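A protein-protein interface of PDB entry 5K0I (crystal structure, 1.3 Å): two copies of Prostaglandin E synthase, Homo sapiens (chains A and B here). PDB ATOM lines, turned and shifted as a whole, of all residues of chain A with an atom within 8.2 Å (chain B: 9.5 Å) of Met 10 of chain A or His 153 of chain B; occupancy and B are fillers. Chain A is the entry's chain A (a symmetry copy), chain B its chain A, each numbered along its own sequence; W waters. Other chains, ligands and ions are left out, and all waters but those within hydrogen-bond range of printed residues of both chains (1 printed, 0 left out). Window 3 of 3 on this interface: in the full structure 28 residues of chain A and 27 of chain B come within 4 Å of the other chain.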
ATOM      1  N   SER A   7      -6.570 -27.764   7.877  1.00  0.00           N
ATOM      2  CA  SER A   7      -7.259 -27.141   6.709  1.00  0.00           C
ATOM      3  C   SER A   7      -7.545 -28.165   5.613  1.00  0.00           C
ATOM      4  O   SER A   7      -6.790 -29.125   5.434  1.00  0.00           O
ATOM      5  CB  SER A   7      -6.428 -25.983   6.153  1.00  0.00           C
ATOM      6  OG  SER A   7      -7.095 -25.335   5.082  1.00  0.00           O
ATOM      7  N   LEU A   8      -8.635 -27.944   4.878  1.00  0.00           N
ATOM      8  CA  LEU A   8      -9.061 -28.852   3.810  1.00  0.00           C
ATOM      9  C   LEU A   8      -8.285 -28.656   2.499  1.00  0.00           C
ATOM     10  O   LEU A   8      -8.509 -29.380   1.526  1.00  0.00           O
ATOM     11  CB  LEU A   8     -10.573 -28.746   3.569  1.00  0.00           C
ATOM     12  CG  LEU A   8     -11.503 -29.340   4.635  1.00  0.00           C
ATOM     13  CD1 LEU A   8     -11.904 -28.295   5.673  1.00  0.00           C
ATOM     14  CD2 LEU A   8     -12.742 -29.936   3.988  1.00  0.00           C
ATOM     15  N   VAL A   9      -7.371 -27.684   2.486  1.00  0.00           N
ATOM     16  CA  VAL A   9      -6.460 -27.469   1.355  1.00  0.00           C
ATOM     17  C   VAL A   9      -5.477 -28.642   1.212  1.00  0.00           C
ATOM     18  O   VAL A   9      -4.918 -28.868   0.135  1.00  0.00           O
ATOM     19  CB  VAL A   9      -5.698 -26.117   1.487  1.00  0.00           C
ATOM     20  CG1 VAL A   9      -4.766 -25.887   0.308  1.00  0.00           C
ATOM     21  CG2 VAL A   9      -6.680 -24.972   1.585  1.00  0.00           C
ATOM     22  N   MET A  10      -5.294 -29.394   2.296  1.00  0.00           N
ATOM     23  CA  MET A  10      -4.411 -30.562   2.295  1.00  0.00           C
ATOM     24  C   MET A  10      -5.138 -31.893   2.070  1.00  0.00           C
ATOM     25  O   MET A  10      -4.624 -32.956   2.430  1.00  0.00           O
ATOM     26  CB  MET A  10      -3.586 -30.611   3.582  1.00  0.00           C
ATOM     27  CG  MET A  10      -2.366 -29.711   3.550  1.00  0.00           C
ATOM     28  SD  MET A  10      -1.363 -29.837   5.036  1.00  0.00           S
ATOM     29  CE  MET A  10      -0.598 -31.444   4.819  1.00  0.00           C
ATOM     30  N   SER A  11      -6.322 -31.827   1.458  1.00  0.00           N
ATOM     31  CA  SER A  11      -7.094 -33.021   1.105  1.00  0.00           C
ATOM     32  C   SER A  11      -6.330 -33.930   0.137  1.00  0.00           C
ATOM     33  O   SER A  11      -6.602 -35.134   0.059  1.00  0.00           O
ATOM     34  CB  SER A  11      -8.447 -32.626   0.511  1.00  0.00           C
ATOM     35  OG  SER A  11      -9.227 -31.926   1.466  1.00  0.00           O
ATOM     36  N   SER A  12      -5.393 -33.328  -0.599  1.00  0.00           N
ATOM     37  CA  SER A  12      -4.491 -34.056  -1.488  1.00  0.00           C
ATOM     38  C   SER A  12      -3.187 -33.270  -1.660  1.00  0.00           C
ATOM     39  O   SER A  12      -3.200 -32.044  -1.633  1.00  0.00           O
ATOM     40  CB  SER A  12      -5.152 -34.301  -2.844  1.00  0.00           C
ATOM     41  OG  SER A  12      -5.186 -33.116  -3.617  1.00  0.00           O
ATOM     42  N   PRO A  13      -2.044 -33.978  -1.832  1.00  0.00           N
ATOM     43  CA  PRO A  13      -0.760 -33.261  -1.930  1.00  0.00           C
ATOM     44  C   PRO A  13      -0.652 -32.223  -3.062  1.00  0.00           C
ATOM     45  O   PRO A  13       0.082 -31.250  -2.924  1.00  0.00           O
ATOM     46  CB  PRO A  13       0.258 -34.389  -2.147  1.00  0.00           C
ATOM     47  CG  PRO A  13      -0.382 -35.589  -1.562  1.00  0.00           C
ATOM     48  CD  PRO A  13      -1.845 -35.444  -1.835  1.00  0.00           C
ATOM     49  N   ALA A  14      -1.380 -32.432  -4.158  1.00  0.00           N
ATOM     50  CA  ALA A  14      -1.326 -31.531  -5.320  1.00  0.00           C
ATOM     51  C   ALA A  14      -2.257 -30.328  -5.191  1.00  0.00           C
ATOM     52  O   ALA A  14      -2.143 -29.358  -5.956  1.00  0.00           O
ATOM     53  CB  ALA A  14      -1.670 -32.300  -6.585  1.00  0.00           C
ATOM     54  N   LEU A  15      -3.185 -30.397  -4.248  1.00  0.00           N
ATOM     55  CA  LEU A  15      -4.241 -29.398  -4.166  1.00  0.00           C
ATOM     56  C   LEU A  15      -3.759 -27.963  -3.909  1.00  0.00           C
ATOM     57  O   LEU A  15      -4.236 -27.046  -4.576  1.00  0.00           O
ATOM     58  CB  LEU A  15      -5.324 -29.822  -3.166  1.00  0.00           C
ATOM     59  CG  LEU A  15      -6.622 -29.015  -3.174  1.00  0.00           C
ATOM     60  CD1 LEU A  15      -7.331 -29.099  -4.534  1.00  0.00           C
ATOM     61  CD2 LEU A  15      -7.542 -29.496  -2.061  1.00  0.00           C
ATOM     62  N   PRO A  16      -2.830 -27.746  -2.951  1.00  0.00           N
ATOM     63  CA  PRO A  16      -2.376 -26.367  -2.742  1.00  0.00           C
ATOM     64  C   PRO A  16      -1.800 -25.730  -4.007  1.00  0.00           C
ATOM     65  O   PRO A  16      -2.122 -24.582  -4.309  1.00  0.00           O
ATOM     66  CB  PRO A  16      -1.293 -26.515  -1.654  1.00  0.00           C
ATOM     67  CG  PRO A  16      -1.698 -27.731  -0.899  1.00  0.00           C
ATOM     68  CD  PRO A  16      -2.277 -28.664  -1.930  1.00  0.00           C
ATOM     69  N   ALA A  17      -0.981 -26.474  -4.744  1.00  0.00           N
ATOM     70  CA  ALA A  17      -0.411 -25.967  -5.989  1.00  0.00           C
ATOM     71  C   ALA A  17      -1.503 -25.656  -7.015  1.00  0.00           C
ATOM     72  O   ALA A  17      -1.451 -24.624  -7.692  1.00  0.00           O
ATOM     73  CB  ALA A  17       0.561 -26.960  -6.570  1.00  0.00           C
ATOM     74  N   LEU A  19      -4.673 -24.875  -6.385  1.00  0.00           N
ATOM     75  CA  LEU A  19      -5.440 -23.720  -5.923  1.00  0.00           C
ATOM     76  C   LEU A  19      -4.675 -22.410  -6.115  1.00  0.00           C
ATOM     77  O   LEU A  19      -5.272 -21.389  -6.463  1.00  0.00           O
ATOM     78  CB  LEU A  19      -5.878 -23.904  -4.466  1.00  0.00           C
ATOM     79  CG  LEU A  19      -6.905 -25.023  -4.248  1.00  0.00           C
ATOM     80  CD1 LEU A  19      -7.181 -25.169  -2.754  1.00  0.00           C
ATOM     81  CD2 LEU A  19      -8.206 -24.794  -5.029  1.00  0.00           C
ATOM     82  N   PHE A  93      -7.156 -34.890  -7.225  1.00  0.00           N
ATOM     83  CA  PHE A  93      -7.642 -35.980  -6.360  1.00  0.00           C
ATOM     84  C   PHE A  93      -7.407 -37.383  -6.923  1.00  0.00           C
ATOM     85  O   PHE A  93      -7.869 -38.380  -6.346  1.00  0.00           O
ATOM     86  CB  PHE A  93      -9.118 -35.772  -6.014  1.00  0.00           C
ATOM     87  CG  PHE A  93      -9.357 -34.616  -5.090  1.00  0.00           C
ATOM     88  CD1 PHE A  93      -9.183 -34.757  -3.713  1.00  0.00           C
ATOM     89  CD2 PHE A  93      -9.751 -33.381  -5.585  1.00  0.00           C
ATOM     90  CE1 PHE A  93      -9.396 -33.680  -2.856  1.00  0.00           C
ATOM     91  CE2 PHE A  93      -9.972 -32.305  -4.736  1.00  0.00           C
ATOM     92  CZ  PHE A  93      -9.793 -32.454  -3.366  1.00  0.00           C
ATOM     93  N   TRP A 102       2.565 -30.546 -10.193  1.00  0.00           N
ATOM     94  CA  TRP A 102       3.090 -29.180 -10.170  1.00  0.00           C
ATOM     95  C   TRP A 102       3.484 -28.722 -11.569  1.00  0.00           C
ATOM     96  O   TRP A 102       3.176 -27.599 -11.973  1.00  0.00           O
ATOM     97  CB  TRP A 102       4.298 -29.066  -9.229  1.00  0.00           C
ATOM     98  CG  TRP A 102       3.987 -29.367  -7.794  1.00  0.00           C
ATOM     99  CD1 TRP A 102       2.770 -29.286  -7.185  1.00  0.00           C
ATOM    100  CD2 TRP A 102       4.916 -29.777  -6.781  1.00  0.00           C
ATOM    101  NE1 TRP A 102       2.880 -29.629  -5.855  1.00  0.00           N
ATOM    102  CE2 TRP A 102       4.187 -29.936  -5.585  1.00  0.00           C
ATOM    103  CE3 TRP A 102       6.292 -30.031  -6.771  1.00  0.00           C
ATOM    104  CZ2 TRP A 102       4.788 -30.335  -4.391  1.00  0.00           C
ATOM    105  CZ3 TRP A 102       6.885 -30.428  -5.586  1.00  0.00           C
ATOM    106  CH2 TRP A 102       6.134 -30.576  -4.412  1.00  0.00           C
ATOM    107  N   PHE B  93     -14.762 -24.012   1.981  1.00  0.00           N
ATOM    108  CA  PHE B  93     -14.003 -25.032   2.726  1.00  0.00           C
ATOM    109  C   PHE B  93     -12.795 -24.486   3.490  1.00  0.00           C
ATOM    110  O   PHE B  93     -12.011 -25.257   4.064  1.00  0.00           O
ATOM    111  CB  PHE B  93     -13.590 -26.176   1.797  1.00  0.00           C
ATOM    112  CG  PHE B  93     -14.739 -27.024   1.345  1.00  0.00           C
ATOM    113  CD1 PHE B  93     -15.243 -28.036   2.163  1.00  0.00           C
ATOM    114  CD2 PHE B  93     -15.331 -26.816   0.107  1.00  0.00           C
ATOM    115  CE1 PHE B  93     -16.318 -28.817   1.746  1.00  0.00           C
ATOM    116  CE2 PHE B  93     -16.399 -27.596  -0.317  1.00  0.00           C
ATOM    117  CZ  PHE B  93     -16.895 -28.600   0.505  1.00  0.00           C
ATOM    118  N   LEU B  94     -12.650 -23.167   3.521  1.00  0.00           N
ATOM    119  CA  LEU B  94     -11.533 -22.543   4.239  1.00  0.00           C
ATOM    120  C   LEU B  94     -11.915 -22.129   5.660  1.00  0.00           C
ATOM    121  O   LEU B  94     -11.192 -21.370   6.308  1.00  0.00           O
ATOM    122  CB  LEU B  94     -10.985 -21.338   3.468  1.00  0.00           C
ATOM    123  CG  LEU B  94     -10.574 -21.500   2.002  1.00  0.00           C
ATOM    124  CD1 LEU B  94     -10.004 -20.185   1.508  1.00  0.00           C
ATOM    125  CD2 LEU B  94      -9.572 -22.626   1.793  1.00  0.00           C
ATOM    126  N   GLN B 145      -8.003 -14.550  -0.112  1.00  0.00           N
ATOM    127  CA  GLN B 145      -8.011 -15.518   0.991  1.00  0.00           C
ATOM    128  C   GLN B 145      -7.541 -16.893   0.540  1.00  0.00           C
ATOM    129  O   GLN B 145      -6.782 -17.562   1.246  1.00  0.00           O
ATOM    130  CB  GLN B 145      -9.385 -15.592   1.652  1.00  0.00           C
ATOM    131  CG  GLN B 145      -9.763 -14.316   2.400  1.00  0.00           C
ATOM    132  CD  GLN B 145     -11.157 -14.361   2.993  1.00  0.00           C
ATOM    133  OE1 GLN B 145     -11.437 -15.154   3.896  1.00  0.00           O
ATOM    134  NE2 GLN B 145     -12.042 -13.500   2.492  1.00  0.00           N
ATOM    135  N   ILE B 146      -7.995 -17.319  -0.637  1.00  0.00           N
ATOM    136  CA  ILE B 146      -7.555 -18.590  -1.208  1.00  0.00           C
ATOM    137  C   ILE B 146      -6.051 -18.574  -1.494  1.00  0.00           C
ATOM    138  O   ILE B 146      -5.357 -19.557  -1.222  1.00  0.00           O
ATOM    139  CB  ILE B 146      -8.361 -18.962  -2.482  1.00  0.00           C
ATOM    140  CG1 ILE B 146      -9.833 -19.182  -2.125  1.00  0.00           C
ATOM    141  CG2 ILE B 146      -7.782 -20.216  -3.133  1.00  0.00           C
ATOM    142  CD1 ILE B 146     -10.775 -19.152  -3.342  1.00  0.00           C
ATOM    143  N   LEU B 147      -5.553 -17.470  -2.052  1.00  0.00           N
ATOM    144  CA  LEU B 147      -4.120 -17.328  -2.327  1.00  0.00           C
ATOM    145  C   LEU B 147      -3.286 -17.569  -1.083  1.00  0.00           C
ATOM    146  O   LEU B 147      -2.321 -18.333  -1.120  1.00  0.00           O
ATOM    147  CB  LEU B 147      -3.784 -15.936  -2.865  1.00  0.00           C
ATOM    148  CG  LEU B 147      -4.008 -15.571  -4.325  1.00  0.00           C
ATOM    149  CD1 LEU B 147      -3.370 -14.212  -4.580  1.00  0.00           C
ATOM    150  CD2 LEU B 147      -3.425 -16.619  -5.270  1.00  0.00           C
ATOM    151  N   TRP B 148      -3.655 -16.913   0.019  1.00  0.00           N
ATOM    152  CA  TRP B 148      -2.887 -17.051   1.265  1.00  0.00           C
ATOM    153  C   TRP B 148      -2.936 -18.465   1.799  1.00  0.00           C
ATOM    154  O   TRP B 148      -1.909 -19.009   2.223  1.00  0.00           O
ATOM    155  CB  TRP B 148      -3.349 -16.088   2.367  1.00  0.00           C
ATOM    156  CG  TRP B 148      -3.549 -14.659   1.958  1.00  0.00           C
ATOM    157  CD1 TRP B 148      -4.507 -13.813   2.433  1.00  0.00           C
ATOM    158  CD2 TRP B 148      -2.791 -13.911   0.998  1.00  0.00           C
ATOM    159  NE1 TRP B 148      -4.397 -12.591   1.837  1.00  0.00           N
ATOM    160  CE2 TRP B 148      -3.361 -12.619   0.943  1.00  0.00           C
ATOM    161  CE3 TRP B 148      -1.695 -14.205   0.173  1.00  0.00           C
ATOM    162  CZ2 TRP B 148      -2.869 -11.618   0.100  1.00  0.00           C
ATOM    163  CZ3 TRP B 148      -1.210 -13.204  -0.676  1.00  0.00           C
ATOM    164  CH2 TRP B 148      -1.796 -11.927  -0.693  1.00  0.00           C
ATOM    165  N   GLU B 149      -4.127 -19.063   1.786  1.00  0.00           N
ATOM    166  CA  GLU B 149      -4.302 -20.418   2.310  1.00  0.00           C
ATOM    167  C   GLU B 149      -3.553 -21.433   1.461  1.00  0.00           C
ATOM    168  O   GLU B 149      -2.886 -22.324   1.988  1.00  0.00           O
ATOM    169  CB  GLU B 149      -5.781 -20.798   2.403  1.00  0.00           C
ATOM    170  CG  GLU B 149      -6.540 -20.118   3.530  1.00  0.00           C
ATOM    171  CD  GLU B 149      -5.952 -20.398   4.901  1.00  0.00           C
ATOM    172  OE1 GLU B 149      -5.907 -19.462   5.725  1.00  0.00           O
ATOM    173  OE2 GLU B 149      -5.531 -21.545   5.157  1.00  0.00           O
ATOM    174  N   ALA B 150      -3.664 -21.307   0.136  1.00  0.00           N
ATOM    175  CA  ALA B 150      -2.943 -22.204  -0.764  1.00  0.00           C
ATOM    176  C   ALA B 150      -1.419 -22.043  -0.630  1.00  0.00           C
ATOM    177  O   ALA B 150      -0.693 -23.034  -0.463  1.00  0.00           O
ATOM    178  CB  ALA B 150      -3.402 -21.994  -2.210  1.00  0.00           C
ATOM    179  N   ALA B 151      -0.943 -20.800  -0.677  1.00  0.00           N
ATOM    180  CA  ALA B 151       0.494 -20.515  -0.597  1.00  0.00           C
ATOM    181  C   ALA B 151       1.129 -21.049   0.684  1.00  0.00           C
ATOM    182  O   ALA B 151       2.246 -21.576   0.650  1.00  0.00           O
ATOM    183  CB  ALA B 151       0.756 -19.022  -0.720  1.00  0.00           C
ATOM    184  N   ARG B 152       0.420 -20.928   1.802  1.00  0.00           N
ATOM    185  CA  ARG B 152       0.982 -21.320   3.095  1.00  0.00           C
ATOM    186  C   ARG B 152       1.017 -22.842   3.291  1.00  0.00           C
ATOM    187  O   ARG B 152       1.669 -23.333   4.216  1.00  0.00           O
ATOM    188  CB  ARG B 152       0.263 -20.600   4.243  1.00  0.00           C
ATOM    189  CG  ARG B 152      -1.027 -21.230   4.721  1.00  0.00           C
ATOM    190  CD  ARG B 152      -1.707 -20.340   5.753  1.00  0.00           C
ATOM    191  NE  ARG B 152      -2.829 -21.009   6.401  1.00  0.00           N
ATOM    192  CZ  ARG B 152      -2.721 -21.888   7.395  1.00  0.00           C
ATOM    193  NH1 ARG B 152      -1.527 -22.205   7.893  1.00  0.00           N
ATOM    194  NH2 ARG B 152      -3.810 -22.448   7.904  1.00  0.00           N
ATOM    195  N   HIS B 153       0.335 -23.575   2.405  1.00  0.00           N
ATOM    196  CA  HIS B 153       0.326 -25.037   2.449  1.00  0.00           C
ATOM    197  C   HIS B 153       1.258 -25.664   1.412  1.00  0.00           C
ATOM    198  O   HIS B 153       1.265 -26.887   1.237  1.00  0.00           O
ATOM    199  CB  HIS B 153      -1.099 -25.575   2.286  1.00  0.00           C
ATOM    200  CG  HIS B 153      -1.948 -25.418   3.508  1.00  0.00           C
ATOM    201  ND1 HIS B 153      -2.667 -24.274   3.773  1.00  0.00           N
ATOM    202  CD2 HIS B 153      -2.197 -26.264   4.537  1.00  0.00           C
ATOM    203  CE1 HIS B 153      -3.320 -24.419   4.914  1.00  0.00           C
ATOM    204  NE2 HIS B 153      -3.052 -25.620   5.396  1.00  0.00           N
ATOM    205  N   LEU B 154       2.055 -24.838   0.740  1.00  0.00           N
ATOM    206  CA  LEU B 154       3.001 -25.337  -0.263  1.00  0.00           C
ATOM    207  C   LEU B 154       4.213 -25.986   0.388  1.00  0.00           C
ATOM    208  O   LEU B 154       4.780 -25.445   1.338  1.00  0.00           O
ATOM    209  CB  LEU B 154       3.451 -24.219  -1.205  1.00  0.00           C
ATOM    210  CG  LEU B 154       2.411 -23.587  -2.131  1.00  0.00           C
ATOM    211  CD1 LEU B 154       3.028 -22.413  -2.877  1.00  0.00           C
ATOM    212  CD2 LEU B 154       1.842 -24.605  -3.109  1.00  0.00           C
ATOM    213  OXT LEU B 154       4.644 -27.063  -0.028  1.00  0.00           O
HETATM  214  O   HOH W   1      -9.981 -25.228   5.961  1.00  0.00           O
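The backbone carbonyl oxygen (O) of Leu 8 of chain A is in hydrogen-bond range of the side-chain hydroxyl (OG) of Ser 11 of chain A.
The backbone carbonyl oxygen (O) of Glu 149 of chain B is in hydrogen-bond range of a ring nitrogen (ND1) of His 153 of chain B (2.7 Å).
Among the printed residues, merely in contact across the chains: Leu 8 of chain A with Phe 93 of chain B (3.4 Å), Ser 7 of chain A with His 153 of chain B (3.5 Å), Pro 16 of chain A with Ala 150 of chain B (3.6 Å), Met 10 of chain A with His 153 of chain B (3.6 Å), Val 9 of chain A with Leu 94 of chain B (3.7 Å), Pro 16 of chain A with His 153 of chain B (3.7 Å), Ala 17 of chain A with Leu 154 of chain B (3.8 Å), Leu 19 of chain A with Ala 150 of chain B (3.9 Å) and Pro 16 of chain A with Leu 154 of chain B (3.9 Å).
Of the printed residues of chain B, Leu 8 of chain A touches Phe 93.
Of the printed residues of chain B, Met 10 of chain A touches His 153.
Of the printed residues of chain B, Leu 19 of chain A touches Ala 150 (3.9 Å).
Of the printed residues of chain A, Phe 93 of chain B touches Leu 8 (3.4 Å).
Leu 147 of chain B touches none of the printed residues of chain A.
Printed residues of chain A within 4 Å of His 153 of chain B: Ser 7, Met 10 and Pro 16.
The nearest printed residue of chain A that does not touch His 153 of chain B is Val 9 of chain A (4.2 Å).
Hydrophobic or aromatic side chains of chain A within 4 Å of the printed part of chain B: Leu 8, Val 9, Met 10, Pro 16 and Leu 19.
Hydrophobic or aromatic side chains of chain B within 4 Å of the printed part of chain A: Phe 93, Leu 94, Ala 150, His 153 and Leu 154.
Among the printed residues, 9 pairs touch across the chains.
Position printed for both chains: 93.
Of the 9 pairs that touch across the chains among the printed residues, none has its exchanged pair printed and touching as well.
Water W1 lies within hydrogen-bond range of the backbone carbonyl oxygen of Phe 93 of chain B (2.8 Å), the side-chain hydroxyl of Ser 7 of chain A (3.0 Å) and the backbone NH of Leu 8 of chain A (3.2 Å).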
